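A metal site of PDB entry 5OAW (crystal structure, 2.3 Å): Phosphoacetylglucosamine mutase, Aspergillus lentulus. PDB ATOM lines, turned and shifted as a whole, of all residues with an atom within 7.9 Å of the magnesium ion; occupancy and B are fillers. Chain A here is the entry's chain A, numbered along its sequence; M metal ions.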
ATOM      1  N   ARG A  33     -27.565  36.885  22.018  1.00  0.00           N
ATOM      2  CA  ARG A  33     -26.239  36.331  22.339  1.00  0.00           C
ATOM      3  C   ARG A  33     -25.383  37.300  23.168  1.00  0.00           C
ATOM      4  O   ARG A  33     -24.993  38.377  22.712  1.00  0.00           O
ATOM      5  CB  ARG A  33     -25.498  35.913  21.066  1.00  0.00           C
ATOM      6  CG  ARG A  33     -24.517  34.779  21.321  1.00  0.00           C
ATOM      7  CD  ARG A  33     -23.698  34.459  20.085  1.00  0.00           C
ATOM      8  NE  ARG A  33     -24.378  33.528  19.171  1.00  0.00           N
ATOM      9  CZ  ARG A  33     -23.818  33.038  18.068  1.00  0.00           C
ATOM     10  NH1 ARG A  33     -22.586  33.375  17.720  1.00  0.00           N
ATOM     11  NH2 ARG A  33     -24.502  32.205  17.295  1.00  0.00           N
ATOM     12  N   THR A  67     -27.434  28.084  22.478  1.00  0.00           N
ATOM     13  CA  THR A  67     -26.004  28.055  22.105  1.00  0.00           C
ATOM     14  C   THR A  67     -25.399  29.413  21.783  1.00  0.00           C
ATOM     15  O   THR A  67     -26.062  30.264  21.207  1.00  0.00           O
ATOM     16  CB  THR A  67     -25.711  27.087  20.919  1.00  0.00           C
ATOM     17  OG1 THR A  67     -24.295  26.868  20.834  1.00  0.00           O
ATOM     18  CG2 THR A  67     -26.221  27.634  19.574  1.00  0.00           C
ATOM     19  N   ALA A  68     -24.134  29.617  22.130  1.00  0.00           N
ATOM     20  CA  ALA A  68     -23.432  30.833  21.696  1.00  0.00           C
ATOM     21  C   ALA A  68     -22.408  30.553  20.609  1.00  0.00           C
ATOM     22  O   ALA A  68     -21.667  31.469  20.199  1.00  0.00           O
ATOM     23  CB  ALA A  68     -22.811  31.568  22.877  1.00  0.00           C
ATOM     24  N   SEP A  69     -22.366  29.295  20.150  1.00  0.00           N
ATOM     25  CA  SEP A  69     -21.627  28.862  18.942  1.00  0.00           C
ATOM     26  CB  SEP A  69     -22.148  29.626  17.693  1.00  0.00           C
ATOM     27  OG  SEP A  69     -21.233  29.647  16.583  1.00  0.00           O
ATOM     28  C   SEP A  69     -20.136  28.878  19.202  1.00  0.00           C
ATOM     29  O   SEP A  69     -19.643  28.021  19.953  1.00  0.00           O
ATOM     30  P   SEP A  69     -21.392  30.639  15.283  1.00  0.00           P
ATOM     31  O1P SEP A  69     -20.132  31.481  15.196  1.00  0.00           O
ATOM     32  O2P SEP A  69     -22.592  31.528  15.529  1.00  0.00           O
ATOM     33  O3P SEP A  69     -21.557  29.645  14.140  1.00  0.00           O
ATOM     34  N   HIS A  70     -19.406  29.832  18.591  1.00  0.00           N
ATOM     35  CA  HIS A  70     -17.944  29.970  18.707  1.00  0.00           C
ATOM     36  C   HIS A  70     -17.492  30.769  19.934  1.00  0.00           C
ATOM     37  O   HIS A  70     -16.315  30.732  20.292  1.00  0.00           O
ATOM     38  CB  HIS A  70     -17.327  30.537  17.413  1.00  0.00           C
ATOM     39  CG  HIS A  70     -17.298  32.038  17.347  1.00  0.00           C
ATOM     40  ND1 HIS A  70     -18.252  32.779  16.682  1.00  0.00           N
ATOM     41  CD2 HIS A  70     -16.426  32.935  17.865  1.00  0.00           C
ATOM     42  CE1 HIS A  70     -17.971  34.066  16.794  1.00  0.00           C
ATOM     43  NE2 HIS A  70     -16.862  34.195  17.508  1.00  0.00           N
ATOM     44  N   ASN A  71     -18.423  31.502  20.553  1.00  0.00           N
ATOM     45  CA  ASN A  71     -18.139  32.333  21.725  1.00  0.00           C
ATOM     46  C   ASN A  71     -17.533  31.562  22.891  1.00  0.00           C
ATOM     47  O   ASN A  71     -17.747  30.350  23.009  1.00  0.00           O
ATOM     48  CB  ASN A  71     -19.400  33.053  22.195  1.00  0.00           C
ATOM     49  CG  ASN A  71     -19.817  34.182  21.262  1.00  0.00           C
ATOM     50  OD1 ASN A  71     -19.610  34.116  20.059  1.00  0.00           O
ATOM     51  ND2 ASN A  71     -20.416  35.207  21.827  1.00  0.00           N
ATOM     52  N   LYS A  79     -31.822  30.894  19.906  1.00  0.00           N
ATOM     53  CA  LYS A  79     -32.248  31.095  18.518  1.00  0.00           C
ATOM     54  C   LYS A  79     -33.575  30.350  18.235  1.00  0.00           C
ATOM     55  O   LYS A  79     -33.762  29.225  18.706  1.00  0.00           O
ATOM     56  CB  LYS A  79     -31.180  30.570  17.557  1.00  0.00           C
ATOM     57  CG  LYS A  79     -29.806  31.221  17.630  1.00  0.00           C
ATOM     58  CD  LYS A  79     -28.887  30.472  18.598  1.00  0.00           C
ATOM     59  CE  LYS A  79     -27.505  31.124  18.652  1.00  0.00           C
ATOM     60  NZ  LYS A  79     -27.365  32.295  19.577  1.00  0.00           N
ATOM     61  N   THR A 164     -26.258  22.119  16.595  1.00  0.00           N
ATOM     62  CA  THR A 164     -27.256  23.017  16.044  1.00  0.00           C
ATOM     63  C   THR A 164     -27.995  22.371  14.832  1.00  0.00           C
ATOM     64  O   THR A 164     -29.222  22.399  14.791  1.00  0.00           O
ATOM     65  CB  THR A 164     -26.680  24.450  15.808  1.00  0.00           C
ATOM     66  OG1 THR A 164     -26.639  25.130  17.066  1.00  0.00           O
ATOM     67  CG2 THR A 164     -27.518  25.301  14.813  1.00  0.00           C
ATOM     68  N   PRO A 165     -27.250  21.739  13.877  1.00  0.00           N
ATOM     69  CA  PRO A 165     -27.968  21.196  12.698  1.00  0.00           C
ATOM     70  C   PRO A 165     -28.930  20.061  12.993  1.00  0.00           C
ATOM     71  O   PRO A 165     -29.915  19.935  12.280  1.00  0.00           O
ATOM     72  CB  PRO A 165     -26.837  20.677  11.821  1.00  0.00           C
ATOM     73  CG  PRO A 165     -25.649  21.480  12.217  1.00  0.00           C
ATOM     74  CD  PRO A 165     -25.794  21.644  13.691  1.00  0.00           C
ATOM     75  N   ASN A 254     -14.159  25.980  22.648  1.00  0.00           N
ATOM     76  CA  ASN A 254     -13.511  26.892  21.669  1.00  0.00           C
ATOM     77  C   ASN A 254     -12.143  27.477  22.100  1.00  0.00           C
ATOM     78  O   ASN A 254     -11.673  28.410  21.470  1.00  0.00           O
ATOM     79  CB  ASN A 254     -14.463  28.026  21.251  1.00  0.00           C
ATOM     80  CG  ASN A 254     -15.786  27.515  20.720  1.00  0.00           C
ATOM     81  OD1 ASN A 254     -15.848  26.832  19.684  1.00  0.00           O
ATOM     82  ND2 ASN A 254     -16.864  27.851  21.411  1.00  0.00           N
ATOM     83  N   LEU A 283     -14.350  21.746  13.509  1.00  0.00           N
ATOM     84  CA  LEU A 283     -15.757  22.102  13.677  1.00  0.00           C
ATOM     85  C   LEU A 283     -15.798  23.278  14.618  1.00  0.00           C
ATOM     86  O   LEU A 283     -14.885  23.474  15.387  1.00  0.00           O
ATOM     87  CB  LEU A 283     -16.555  20.954  14.298  1.00  0.00           C
ATOM     88  CG  LEU A 283     -16.353  19.484  13.887  1.00  0.00           C
ATOM     89  CD1 LEU A 283     -17.378  18.621  14.629  1.00  0.00           C
ATOM     90  CD2 LEU A 283     -16.453  19.261  12.389  1.00  0.00           C
ATOM     91  N   ASP A 284     -16.875  24.066  14.589  1.00  0.00           N
ATOM     92  CA  ASP A 284     -17.072  25.047  15.655  1.00  0.00           C
ATOM     93  C   ASP A 284     -17.820  24.389  16.823  1.00  0.00           C
ATOM     94  O   ASP A 284     -18.160  23.195  16.751  1.00  0.00           O
ATOM     95  CB  ASP A 284     -17.720  26.348  15.158  1.00  0.00           C
ATOM     96  CG  ASP A 284     -19.143  26.174  14.708  1.00  0.00           C
ATOM     97  OD1 ASP A 284     -19.494  25.093  14.182  1.00  0.00           O
ATOM     98  OD2 ASP A 284     -19.908  27.148  14.845  1.00  0.00           O
ATOM     99  N   GLY A 285     -18.054  25.162  17.891  1.00  0.00           N
ATOM    100  CA  GLY A 285     -18.657  24.656  19.137  1.00  0.00           C
ATOM    101  C   GLY A 285     -20.014  23.981  18.995  1.00  0.00           C
ATOM    102  O   GLY A 285     -20.302  23.024  19.719  1.00  0.00           O
ATOM    103  N   ASP A 286     -20.841  24.457  18.065  1.00  0.00           N
ATOM    104  CA  ASP A 286     -22.182  23.884  17.866  1.00  0.00           C
ATOM    105  C   ASP A 286     -22.275  23.109  16.539  1.00  0.00           C
ATOM    106  O   ASP A 286     -23.370  22.703  16.113  1.00  0.00           O
ATOM    107  CB  ASP A 286     -23.295  24.932  18.011  1.00  0.00           C
ATOM    108  CG  ASP A 286     -23.257  26.013  16.944  1.00  0.00           C
ATOM    109  OD1 ASP A 286     -22.221  26.166  16.253  1.00  0.00           O
ATOM    110  OD2 ASP A 286     -24.274  26.740  16.778  1.00  0.00           O
ATOM    111  N   ALA A 287     -21.105  22.910  15.926  1.00  0.00           N
ATOM    112  CA  ALA A 287     -20.892  22.058  14.759  1.00  0.00           C
ATOM    113  C   ALA A 287     -21.768  22.363  13.531  1.00  0.00           C
ATOM    114  O   ALA A 287     -22.260  21.468  12.856  1.00  0.00           O
ATOM    115  CB  ALA A 287     -20.964  20.572  15.157  1.00  0.00           C
ATOM    116  N   ASP A 288     -21.926  23.654  13.245  1.00  0.00           N
ATOM    117  CA  ASP A 288     -22.485  24.103  11.976  1.00  0.00           C
ATOM    118  C   ASP A 288     -21.452  24.861  11.115  1.00  0.00           C
ATOM    119  O   ASP A 288     -21.815  25.521  10.146  1.00  0.00           O
ATOM    120  CB  ASP A 288     -23.745  24.934  12.216  1.00  0.00           C
ATOM    121  CG  ASP A 288     -23.472  26.245  12.951  1.00  0.00           C
ATOM    122  OD1 ASP A 288     -24.371  27.112  13.004  1.00  0.00           O
ATOM    123  OD2 ASP A 288     -22.364  26.417  13.489  1.00  0.00           O
ATOM    124  N   ARG A 289     -20.175  24.745  11.462  1.00  0.00           N
ATOM    125  CA  ARG A 289     -19.069  25.313  10.676  1.00  0.00           C
ATOM    126  C   ARG A 289     -17.918  24.318  10.637  1.00  0.00           C
ATOM    127  O   ARG A 289     -17.511  23.770  11.660  1.00  0.00           O
ATOM    128  CB  ARG A 289     -18.555  26.631  11.257  1.00  0.00           C
ATOM    129  CG  ARG A 289     -19.478  27.818  11.062  1.00  0.00           C
ATOM    130  CD  ARG A 289     -19.156  28.912  12.068  1.00  0.00           C
ATOM    131  NE  ARG A 289     -17.785  29.348  11.895  1.00  0.00           N
ATOM    132  CZ  ARG A 289     -17.241  30.412  12.464  1.00  0.00           C
ATOM    133  NH1 ARG A 289     -17.950  31.193  13.262  1.00  0.00           N
ATOM    134  NH2 ARG A 289     -15.968  30.698  12.211  1.00  0.00           N
ATOM    135  N   HIS A 384     -19.462  27.832   7.269  1.00  0.00           N
ATOM    136  CA  HIS A 384     -20.906  27.594   7.236  1.00  0.00           C
ATOM    137  C   HIS A 384     -21.412  27.497   5.807  1.00  0.00           C
ATOM    138  O   HIS A 384     -21.188  28.395   4.987  1.00  0.00           O
ATOM    139  CB  HIS A 384     -21.686  28.682   7.972  1.00  0.00           C
ATOM    140  CG  HIS A 384     -23.135  28.357   8.112  1.00  0.00           C
ATOM    141  ND1 HIS A 384     -24.097  28.789   7.208  1.00  0.00           N
ATOM    142  CD2 HIS A 384     -23.795  27.577   8.999  1.00  0.00           C
ATOM    143  CE1 HIS A 384     -25.273  28.311   7.557  1.00  0.00           C
ATOM    144  NE2 HIS A 384     -25.117  27.565   8.640  1.00  0.00           N
ATOM    145  N   GLY A 426     -26.803  24.668   7.100  1.00  0.00           N
ATOM    146  CA  GLY A 426     -25.410  24.255   6.925  1.00  0.00           C
ATOM    147  C   GLY A 426     -24.941  23.475   8.149  1.00  0.00           C
ATOM    148  O   GLY A 426     -25.211  23.870   9.284  1.00  0.00           O
HETATM  149 MG    MG M   1     -21.984  27.816  14.855  1.00  0.00          MG
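The magnesium ion is bound by OD2 of Asp 288 (2.0 Å), O3P of SEP 69 (2.0 Å), OD1 of Asp 286 (2.2 Å) and OD2 of Asp 284 (2.2 Å). The magnesium ion has four donor atoms within binding distance. Slightly farther from the magnesium ion lies OG of SEP 69 (2.6 Å).
Four residues have an atom within 4 Å of the magnesium ion: SEP 69, Asp 284, Asp 286 and Asp 288. The nearest printed residue that does not touch the magnesium ion is Arg 289 (4.1 Å).
O of SEP 69 is in hydrogen-bond range of ND2 of Asn 254, 3.1 Å away. N of SEP 69 is in hydrogen-bond range of the side-chain hydroxyl (OG1) of Thr 67 (3.2 Å). N of Ala 287 sits at hydrogen-bond distance from OD1 of Asp 284 (3.2 Å). The side-chain carboxylate (OD2) of Asp 286 is in hydrogen-bond range of the side-chain hydroxyl (OG1) of Thr 164, 2.9 Å away. O1P of SEP 69 lies within salt-bridge range of the guanidinium group of Arg 289 (2.9 Å). A ring nitrogen (ND1) of His 70 sits at hydrogen-bond distance from O1P of SEP 69, at 2.7 Å. The side-chain carboxylate (OD1) of Asp 284 is in hydrogen-bond range of the backbone NH (N) of Arg 289 (2.8 Å). O2P of SEP 69 is in salt-bridge range of NH2 of Arg 33.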
